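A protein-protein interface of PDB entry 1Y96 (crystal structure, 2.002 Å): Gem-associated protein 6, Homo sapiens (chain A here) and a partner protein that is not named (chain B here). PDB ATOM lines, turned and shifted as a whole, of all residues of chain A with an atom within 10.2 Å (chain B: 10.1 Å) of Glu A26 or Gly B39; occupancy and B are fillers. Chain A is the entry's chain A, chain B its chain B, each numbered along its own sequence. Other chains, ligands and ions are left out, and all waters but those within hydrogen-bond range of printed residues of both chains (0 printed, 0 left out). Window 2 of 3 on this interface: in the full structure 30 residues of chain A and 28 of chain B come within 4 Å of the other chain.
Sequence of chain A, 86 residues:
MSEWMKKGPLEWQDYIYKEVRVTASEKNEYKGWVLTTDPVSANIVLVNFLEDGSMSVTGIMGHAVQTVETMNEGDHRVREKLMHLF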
ATOM      1  N   VAL A  22       8.233  -6.126 -12.479  1.00  0.00           N
ATOM      2  CA  VAL A  22       8.267  -5.012 -13.410  1.00  0.00           C
ATOM      3  C   VAL A  22       6.865  -4.724 -13.893  1.00  0.00           C
ATOM      4  O   VAL A  22       6.167  -5.616 -14.368  1.00  0.00           O
ATOM      5  CB  VAL A  22       9.161  -5.313 -14.658  1.00  0.00           C
ATOM      6  CG1 VAL A  22       9.220  -4.114 -15.582  1.00  0.00           C
ATOM      7  CG2 VAL A  22      10.548  -5.730 -14.241  1.00  0.00           C
ATOM      8  N   THR A  23       6.471  -3.470 -13.789  1.00  0.00           N
ATOM      9  CA  THR A  23       5.241  -2.995 -14.368  1.00  0.00           C
ATOM     10  C   THR A  23       5.620  -2.255 -15.629  1.00  0.00           C
ATOM     11  O   THR A  23       6.579  -1.489 -15.628  1.00  0.00           O
ATOM     12  CB  THR A  23       4.527  -2.057 -13.375  1.00  0.00           C
ATOM     13  OG1 THR A  23       4.030  -2.832 -12.271  1.00  0.00           O
ATOM     14  CG2 THR A  23       3.300  -1.456 -13.987  1.00  0.00           C
ATOM     15  N   ALA A  24       4.860  -2.486 -16.694  1.00  0.00           N
ATOM     16  CA  ALA A  24       5.158  -1.924 -18.008  1.00  0.00           C
ATOM     17  C   ALA A  24       3.885  -1.428 -18.681  1.00  0.00           C
ATOM     18  O   ALA A  24       2.782  -1.678 -18.185  1.00  0.00           O
ATOM     19  CB  ALA A  24       5.859  -2.982 -18.890  1.00  0.00           C
ATOM     20  N   SER A  25       4.050  -0.739 -19.805  1.00  0.00           N
ATOM     21  CA  SER A  25       2.951  -0.171 -20.584  1.00  0.00           C
ATOM     22  C   SER A  25       1.765  -1.126 -20.745  1.00  0.00           C
ATOM     23  O   SER A  25       1.945  -2.343 -20.867  1.00  0.00           O
ATOM     24  CB  SER A  25       3.447   0.224 -21.985  1.00  0.00           C
ATOM     25  OG  SER A  25       4.536   1.133 -21.946  1.00  0.00           O
ATOM     26  N   GLU A  26       0.559  -0.551 -20.760  1.00  0.00           N
ATOM     27  CA  GLU A  26      -0.694  -1.277 -21.011  1.00  0.00           C
ATOM     28  C   GLU A  26      -0.948  -2.398 -20.013  1.00  0.00           C
ATOM     29  O   GLU A  26      -1.389  -3.483 -20.395  1.00  0.00           O
ATOM     30  CB  GLU A  26      -0.731  -1.826 -22.445  1.00  0.00           C
ATOM     31  CG  GLU A  26      -0.512  -0.767 -23.517  1.00  0.00           C
ATOM     32  CD  GLU A  26      -0.671  -1.289 -24.937  1.00  0.00           C
ATOM     33  OE1 GLU A  26      -0.840  -2.515 -25.131  1.00  0.00           O
ATOM     34  OE2 GLU A  26      -0.617  -0.456 -25.874  1.00  0.00           O
ATOM     35  N   LYS A  27      -0.629  -2.142 -18.748  1.00  0.00           N
ATOM     36  CA  LYS A  27      -0.920  -3.061 -17.640  1.00  0.00           C
ATOM     37  C   LYS A  27      -0.207  -4.418 -17.704  1.00  0.00           C
ATOM     38  O   LYS A  27      -0.608  -5.368 -17.033  1.00  0.00           O
ATOM     39  CB  LYS A  27      -2.445  -3.273 -17.505  1.00  0.00           C
ATOM     40  CG  LYS A  27      -3.274  -1.985 -17.621  1.00  0.00           C
ATOM     41  CD  LYS A  27      -4.724  -2.189 -17.136  1.00  0.00           C
ATOM     42  CE  LYS A  27      -5.516  -0.867 -17.118  1.00  0.00           C
ATOM     43  NZ  LYS A  27      -4.944   0.130 -16.148  1.00  0.00           N
ATOM     44  N   ASN A  28       0.860  -4.511 -18.489  1.00  0.00           N
ATOM     45  CA  ASN A  28       1.646  -5.737 -18.551  1.00  0.00           C
ATOM     46  C   ASN A  28       2.524  -5.843 -17.319  1.00  0.00           C
ATOM     47  O   ASN A  28       3.166  -4.867 -16.934  1.00  0.00           O
ATOM     48  CB  ASN A  28       2.488  -5.745 -19.820  1.00  0.00           C
ATOM     49  CG  ASN A  28       1.666  -6.049 -21.044  1.00  0.00           C
ATOM     50  OD1 ASN A  28       1.260  -7.188 -21.241  1.00  0.00           O
ATOM     51  ND2 ASN A  28       1.418  -5.039 -21.874  1.00  0.00           N
ATOM     52  N   GLU A  29       2.530  -7.015 -16.690  1.00  0.00           N
ATOM     53  CA  GLU A  29       3.292  -7.248 -15.469  1.00  0.00           C
ATOM     54  C   GLU A  29       4.193  -8.451 -15.632  1.00  0.00           C
ATOM     55  O   GLU A  29       3.829  -9.413 -16.286  1.00  0.00           O
ATOM     56  CB  GLU A  29       2.348  -7.471 -14.268  1.00  0.00           C
ATOM     57  CG  GLU A  29       2.753  -6.718 -13.003  1.00  0.00           C
ATOM     58  CD  GLU A  29       1.551  -6.326 -12.135  1.00  0.00           C
ATOM     59  OE1 GLU A  29       0.876  -7.237 -11.602  1.00  0.00           O
ATOM     60  OE2 GLU A  29       1.282  -5.110 -11.986  1.00  0.00           O
ATOM     61  N   TYR A  30       5.377  -8.391 -15.032  1.00  0.00           N
ATOM     62  CA  TYR A  30       6.347  -9.477 -15.111  1.00  0.00           C
ATOM     63  C   TYR A  30       6.998  -9.660 -13.767  1.00  0.00           C
ATOM     64  O   TYR A  30       7.107  -8.730 -12.985  1.00  0.00           O
ATOM     65  CB  TYR A  30       7.437  -9.173 -16.163  1.00  0.00           C
ATOM     66  CG  TYR A  30       6.875  -8.768 -17.504  1.00  0.00           C
ATOM     67  CD1 TYR A  30       6.521  -7.459 -17.757  1.00  0.00           C
ATOM     68  CD2 TYR A  30       6.667  -9.716 -18.512  1.00  0.00           C
ATOM     69  CE1 TYR A  30       5.983  -7.087 -18.987  1.00  0.00           C
ATOM     70  CE2 TYR A  30       6.119  -9.359 -19.736  1.00  0.00           C
ATOM     71  CZ  TYR A  30       5.784  -8.047 -19.965  1.00  0.00           C
ATOM     72  OH  TYR A  30       5.246  -7.680 -21.175  1.00  0.00           O
ATOM     73  N   ILE A  60      12.087  -6.750 -21.479  1.00  0.00           N
ATOM     74  CA  ILE A  60      11.060  -5.716 -21.450  1.00  0.00           C
ATOM     75  C   ILE A  60      11.705  -4.422 -21.926  1.00  0.00           C
ATOM     76  O   ILE A  60      12.733  -4.017 -21.389  1.00  0.00           O
ATOM     77  CB  ILE A  60      10.495  -5.579 -20.029  1.00  0.00           C
ATOM     78  CG1 ILE A  60       9.864  -6.922 -19.601  1.00  0.00           C
ATOM     79  CG2 ILE A  60       9.454  -4.469 -19.958  1.00  0.00           C
ATOM     80  CD1 ILE A  60      10.323  -7.388 -18.274  1.00  0.00           C
ATOM     81  N   HIS A  63      11.748   1.762 -22.890  1.00  0.00           N
ATOM     82  CA  HIS A  63      10.706   2.782 -23.073  1.00  0.00           C
ATOM     83  C   HIS A  63       9.340   2.385 -22.481  1.00  0.00           C
ATOM     84  O   HIS A  63       8.511   3.251 -22.237  1.00  0.00           O
ATOM     85  CB  HIS A  63      10.524   3.134 -24.564  1.00  0.00           C
ATOM     86  CG  HIS A  63       9.824   2.076 -25.364  1.00  0.00           C
ATOM     87  ND1 HIS A  63      10.500   1.174 -26.158  1.00  0.00           N
ATOM     88  CD2 HIS A  63       8.509   1.781 -25.501  1.00  0.00           C
ATOM     89  CE1 HIS A  63       9.633   0.370 -26.747  1.00  0.00           C
ATOM     90  NE2 HIS A  63       8.418   0.708 -26.355  1.00  0.00           N
ATOM     91  N   ALA A  64       9.100   1.088 -22.302  1.00  0.00           N
ATOM     92  CA  ALA A  64       7.852   0.582 -21.712  1.00  0.00           C
ATOM     93  C   ALA A  64       7.894   0.351 -20.210  1.00  0.00           C
ATOM     94  O   ALA A  64       6.849   0.106 -19.591  1.00  0.00           O
ATOM     95  CB  ALA A  64       7.423  -0.712 -22.412  1.00  0.00           C
ATOM     96  N   VAL A  65       9.075   0.425 -19.609  1.00  0.00           N
ATOM     97  CA  VAL A  65       9.213   0.162 -18.180  1.00  0.00           C
ATOM     98  C   VAL A  65       8.619   1.338 -17.374  1.00  0.00           C
ATOM     99  O   VAL A  65       8.946   2.495 -17.632  1.00  0.00           O
ATOM    100  CB  VAL A  65      10.687  -0.076 -17.800  1.00  0.00           C
ATOM    101  CG1 VAL A  65      10.868  -0.102 -16.303  1.00  0.00           C
ATOM    102  CG2 VAL A  65      11.199  -1.384 -18.431  1.00  0.00           C
ATOM    103  N   GLN A  66       7.752   1.017 -16.412  1.00  0.00           N
ATOM    104  CA  GLN A  66       7.128   2.015 -15.535  1.00  0.00           C
ATOM    105  C   GLN A  66       7.724   1.946 -14.129  1.00  0.00           C
ATOM    106  O   GLN A  66       8.251   2.940 -13.640  1.00  0.00           O
ATOM    107  CB  GLN A  66       5.600   1.824 -15.490  1.00  0.00           C
ATOM    108  CG  GLN A  66       4.901   2.407 -16.718  1.00  0.00           C
ATOM    109  CD  GLN A  66       3.427   2.052 -16.792  1.00  0.00           C
ATOM    110  OE1 GLN A  66       2.887   1.429 -15.877  1.00  0.00           O
ATOM    111  NE2 GLN A  66       2.775   2.439 -17.883  1.00  0.00           N
ATOM    112  N   PHE B  34       6.420 -11.851 -29.201  1.00  0.00           N
ATOM    113  CA  PHE B  34       6.500 -10.437 -28.976  1.00  0.00           C
ATOM    114  C   PHE B  34       5.153  -9.966 -28.448  1.00  0.00           C
ATOM    115  O   PHE B  34       4.093 -10.314 -29.002  1.00  0.00           O
ATOM    116  CB  PHE B  34       6.859  -9.702 -30.280  1.00  0.00           C
ATOM    117  CG  PHE B  34       8.223 -10.051 -30.812  1.00  0.00           C
ATOM    118  CD1 PHE B  34       8.386 -11.064 -31.729  1.00  0.00           C
ATOM    119  CD2 PHE B  34       9.336  -9.377 -30.368  1.00  0.00           C
ATOM    120  CE1 PHE B  34       9.646 -11.412 -32.190  1.00  0.00           C
ATOM    121  CE2 PHE B  34      10.577  -9.703 -30.822  1.00  0.00           C
ATOM    122  CZ  PHE B  34      10.741 -10.733 -31.740  1.00  0.00           C
ATOM    123  N   THR B  35       5.185  -9.228 -27.351  1.00  0.00           N
ATOM    124  CA  THR B  35       4.018  -8.506 -26.871  1.00  0.00           C
ATOM    125  C   THR B  35       4.098  -7.108 -27.411  1.00  0.00           C
ATOM    126  O   THR B  35       5.054  -6.380 -27.157  1.00  0.00           O
ATOM    127  CB  THR B  35       3.995  -8.498 -25.359  1.00  0.00           C
ATOM    128  OG1 THR B  35       3.864  -9.846 -24.893  1.00  0.00           O
ATOM    129  CG2 THR B  35       2.755  -7.735 -24.821  1.00  0.00           C
ATOM    130  N   LEU B  36       3.091  -6.738 -28.173  1.00  0.00           N
ATOM    131  CA  LEU B  36       3.100  -5.511 -28.931  1.00  0.00           C
ATOM    132  C   LEU B  36       2.180  -4.509 -28.252  1.00  0.00           C
ATOM    133  O   LEU B  36       1.392  -4.862 -27.368  1.00  0.00           O
ATOM    134  CB  LEU B  36       2.624  -5.775 -30.365  1.00  0.00           C
ATOM    135  CG  LEU B  36       3.599  -6.124 -31.488  1.00  0.00           C
ATOM    136  CD1 LEU B  36       4.735  -6.962 -31.021  1.00  0.00           C
ATOM    137  CD2 LEU B  36       2.865  -6.806 -32.667  1.00  0.00           C
ATOM    138  N   HIS B  37       2.321  -3.247 -28.642  1.00  0.00           N
ATOM    139  CA  HIS B  37       1.387  -2.206 -28.230  1.00  0.00           C
ATOM    140  C   HIS B  37       0.073  -2.454 -28.968  1.00  0.00           C
ATOM    141  O   HIS B  37       0.042  -3.213 -29.943  1.00  0.00           O
ATOM    142  CB  HIS B  37       1.961  -0.797 -28.468  1.00  0.00           C
ATOM    143  CG  HIS B  37       2.159  -0.432 -29.912  1.00  0.00           C
ATOM    144  ND1 HIS B  37       2.410   0.864 -30.316  1.00  0.00           N
ATOM    145  CD2 HIS B  37       2.152  -1.182 -31.044  1.00  0.00           C
ATOM    146  CE1 HIS B  37       2.545   0.899 -31.631  1.00  0.00           C
ATOM    147  NE2 HIS B  37       2.386  -0.330 -32.099  1.00  0.00           N
ATOM    148  N   GLU B  38      -1.000  -1.837 -28.480  1.00  0.00           N
ATOM    149  CA  GLU B  38      -2.364  -2.087 -28.952  1.00  0.00           C
ATOM    150  C   GLU B  38      -2.911  -3.480 -28.586  1.00  0.00           C
ATOM    151  O   GLU B  38      -3.833  -3.969 -29.242  1.00  0.00           O
ATOM    152  CB  GLU B  38      -2.469  -1.829 -30.466  1.00  0.00           C
ATOM    153  CG  GLU B  38      -2.033  -0.423 -30.864  1.00  0.00           C
ATOM    154  CD  GLU B  38      -1.596  -0.305 -32.313  1.00  0.00           C
ATOM    155  OE1 GLU B  38      -2.035  -1.125 -33.157  1.00  0.00           O
ATOM    156  OE2 GLU B  38      -0.819   0.630 -32.609  1.00  0.00           O
ATOM    157  N   GLY B  39      -2.353  -4.110 -27.547  1.00  0.00           N
ATOM    158  CA  GLY B  39      -2.839  -5.397 -27.047  1.00  0.00           C
ATOM    159  C   GLY B  39      -2.516  -6.640 -27.883  1.00  0.00           C
ATOM    160  O   GLY B  39      -2.970  -7.737 -27.570  1.00  0.00           O
ATOM    161  N   VAL B  40      -1.720  -6.483 -28.935  1.00  0.00           N
ATOM    162  CA  VAL B  40      -1.468  -7.564 -29.893  1.00  0.00           C
ATOM    163  C   VAL B  40      -0.235  -8.408 -29.526  1.00  0.00           C
ATOM    164  O   VAL B  40       0.703  -7.922 -28.897  1.00  0.00           O
ATOM    165  CB  VAL B  40      -1.252  -6.986 -31.311  1.00  0.00           C
ATOM    166  CG1 VAL B  40      -1.134  -8.101 -32.369  1.00  0.00           C
ATOM    167  CG2 VAL B  40      -2.372  -6.017 -31.665  1.00  0.00           C
ATOM    168  N   ARG B  41      -0.267  -9.669 -29.949  1.00  0.00           N
ATOM    169  CA  ARG B  41       0.827 -10.620 -29.814  1.00  0.00           C
ATOM    170  C   ARG B  41       1.237 -11.082 -31.209  1.00  0.00           C
ATOM    171  O   ARG B  41       0.368 -11.346 -32.032  1.00  0.00           O
ATOM    172  CB  ARG B  41       0.335 -11.852 -29.048  1.00  0.00           C
ATOM    173  CG  ARG B  41       1.125 -12.219 -27.827  1.00  0.00           C
ATOM    174  CD  ARG B  41       0.854 -11.322 -26.631  1.00  0.00           C
ATOM    175  NE  ARG B  41       1.098 -12.007 -25.357  1.00  0.00           N
ATOM    176  CZ  ARG B  41       0.794 -11.505 -24.159  1.00  0.00           C
ATOM    177  NH1 ARG B  41       0.227 -10.302 -24.047  1.00  0.00           N
ATOM    178  NH2 ARG B  41       1.058 -12.209 -23.062  1.00  0.00           N
ATOM    179  N   VAL B  42       2.536 -11.197 -31.480  1.00  0.00           N
ATOM    180  CA  VAL B  42       2.999 -11.893 -32.692  1.00  0.00           C
ATOM    181  C   VAL B  42       4.239 -12.748 -32.417  1.00  0.00           C
ATOM    182  O   VAL B  42       5.023 -12.449 -31.514  1.00  0.00           O
ATOM    183  CB  VAL B  42       3.249 -10.903 -33.859  1.00  0.00           C
ATOM    184  CG1 VAL B  42       4.552 -10.129 -33.673  1.00  0.00           C
ATOM    185  CG2 VAL B  42       3.219 -11.637 -35.226  1.00  0.00           C
ATOM    186  N   SER B  76      10.212   0.371 -30.922  1.00  0.00           N
ATOM    187  CA  SER B  76       9.151   1.275 -30.431  1.00  0.00           C
ATOM    188  C   SER B  76       7.722   0.655 -30.440  1.00  0.00           C
ATOM    189  O   SER B  76       6.870   1.103 -29.685  1.00  0.00           O
ATOM    190  CB  SER B  76       9.148   2.593 -31.209  1.00  0.00           C
ATOM    191  OG  SER B  76       8.852   2.357 -32.570  1.00  0.00           O
ATOM    192  N   ASP B  77       7.462  -0.359 -31.274  1.00  0.00           N
ATOM    193  CA  ASP B  77       6.162  -1.060 -31.277  1.00  0.00           C
ATOM    194  C   ASP B  77       6.092  -2.213 -30.284  1.00  0.00           C
ATOM    195  O   ASP B  77       5.030  -2.812 -30.080  1.00  0.00           O
ATOM    196  CB  ASP B  77       5.840  -1.619 -32.671  1.00  0.00           C
ATOM    197  CG  ASP B  77       5.656  -0.532 -33.711  1.00  0.00           C
ATOM    198  OD1 ASP B  77       5.148   0.551 -33.360  1.00  0.00           O
ATOM    199  OD2 ASP B  77       5.985  -0.665 -34.900  1.00  0.00           O
ATOM    200  N   ILE B  78       7.224  -2.544 -29.675  1.00  0.00           N
ATOM    201  CA  ILE B  78       7.322  -3.732 -28.851  1.00  0.00           C
ATOM    202  C   ILE B  78       7.305  -3.330 -27.391  1.00  0.00           C
ATOM    203  O   ILE B  78       7.950  -2.340 -27.006  1.00  0.00           O
ATOM    204  CB  ILE B  78       8.621  -4.514 -29.196  1.00  0.00           C
ATOM    205  CG1 ILE B  78       8.585  -5.003 -30.650  1.00  0.00           C
ATOM    206  CG2 ILE B  78       8.815  -5.682 -28.251  1.00  0.00           C
ATOM    207  CD1 ILE B  78       9.927  -5.619 -31.140  1.00  0.00           C
ATOM    208  N   ILE B  79       6.602  -4.121 -26.579  1.00  0.00           N
ATOM    209  CA  ILE B  79       6.638  -3.963 -25.125  1.00  0.00           C
ATOM    210  C   ILE B  79       7.586  -4.968 -24.498  1.00  0.00           C
ATOM    211  O   ILE B  79       8.403  -4.608 -23.668  1.00  0.00           O
ATOM    212  CB  ILE B  79       5.217  -4.088 -24.498  1.00  0.00           C
ATOM    213  CG1 ILE B  79       4.416  -2.818 -24.789  1.00  0.00           C
ATOM    214  CG2 ILE B  79       5.288  -4.300 -22.952  1.00  0.00           C
ATOM    215  CD1 ILE B  79       2.916  -2.961 -24.526  1.00  0.00           C
ATOM    216  N   SER B  80       7.427  -6.234 -24.856  1.00  0.00           N
ATOM    217  CA  SER B  80       8.295  -7.287 -24.364  1.00  0.00           C
ATOM    218  C   SER B  80       8.485  -8.361 -25.411  1.00  0.00           C
ATOM    219  O   SER B  80       7.776  -8.382 -26.406  1.00  0.00           O
ATOM    220  CB  SER B  80       7.779  -7.860 -23.028  1.00  0.00           C
ATOM    221  OG  SER B  80       6.553  -8.566 -23.171  1.00  0.00           O
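Of chain B, only Leu B36 (3.9 Å), His B37 (3.6 Å), Glu B38 (3.0 Å), Gly B39 (3.3 Å) and Ile B79 (3.8 Å) come within 4 Å of Glu A26. Gly B39 touches one residue of chain A. Ser A25 touches one residue of chain B. No residue of chain A comes within 4 Å of Val B40. Printed residues of chain A within 4 Å of Ile B78: His A63 (3.2 Å). Printed residues of chain A within 4 Å of Ser B80: Tyr A30 (2.5 Å). Of the printed residues of chain B, Tyr A30 touches Ile B79 and Ser B80. Lys A27 touches none of the printed residues of chain B. The nearest residue of chain B that does not touch Glu A26 is Val B40 (5.6 Å).
The backbone NH (N) of Val A22 lies within hydrogen-bond range of the backbone carbonyl oxygen (O) of Tyr A30 (2.9 Å). The side-chain amide nitrogen of Asn A28 lies within hydrogen-bond range of the backbone carbonyl oxygen of Ser A25 (2.9 Å). The backbone carbonyl oxygen (O) of Ala A64 sits at hydrogen-bond distance from the backbone NH (N) of Ser A25 (2.9 Å). The backbone NH (N) of Thr B35 is in hydrogen-bond range of the backbone carbonyl oxygen (O) of Ser B80, 2.9 Å away. A ring nitrogen (NE2) of His B37 lies within hydrogen-bond range of the side-chain carboxylate (OE2) of Glu B38, 3.4 Å away. The backbone NH of His B37 lies within hydrogen-bond range of the backbone carbonyl oxygen of Asp B77, at 3.1 Å.
The side-chain carboxylate of Glu A26 lies within hydrogen-bond range of the backbone NH of Glu B38 (3.0 Å). The side-chain carboxylate (OE1) of Glu A26 is in hydrogen-bond range of the backbone NH (N) of Gly B39, at 3.3 Å. OH of Tyr A30 is in hydrogen-bond range of OG of Ser B80, at 2.5 Å. A ring nitrogen (NE2) of His A63 sits at hydrogen-bond distance from the backbone carbonyl oxygen (O) of Ile B78, at 3.2 Å.
Of the 14 printed residues of chain A, 6 touch a printed residue of chain B. Printed residues of chain A that touch a printed residue of chain B: Ser A25, Glu A26, Asn A28, Tyr A30, Ile A60 and His A63. Along chain A the printed residues that touch a printed residue of chain B span positions 25 to 63. Among the printed residues, 13 pairs touch across the chains. Among the printed residues, no Asp or Glu carboxylate lies within 4 Å of a Lys or Arg side-chain nitrogen of the other chain.
O of Ser A25 touches CD1 of Ile B79, at 3.8 Å. OE1 of Glu A26 touches O of Leu B36, 3.9 Å away. Glu A26 touches His B37. Ile B79 touches Glu A26 (CD1 to OE1, 3.8 Å). Thr B35 touches Asn A28. Asn A28 touches Ile B79 (ND2 to CD1, 3.7 Å). Tyr A30 touches Ile B79 (OH to CG2, 3.8 Å). Ile A60 touches Ile B79. His A63 touches Ser B76.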
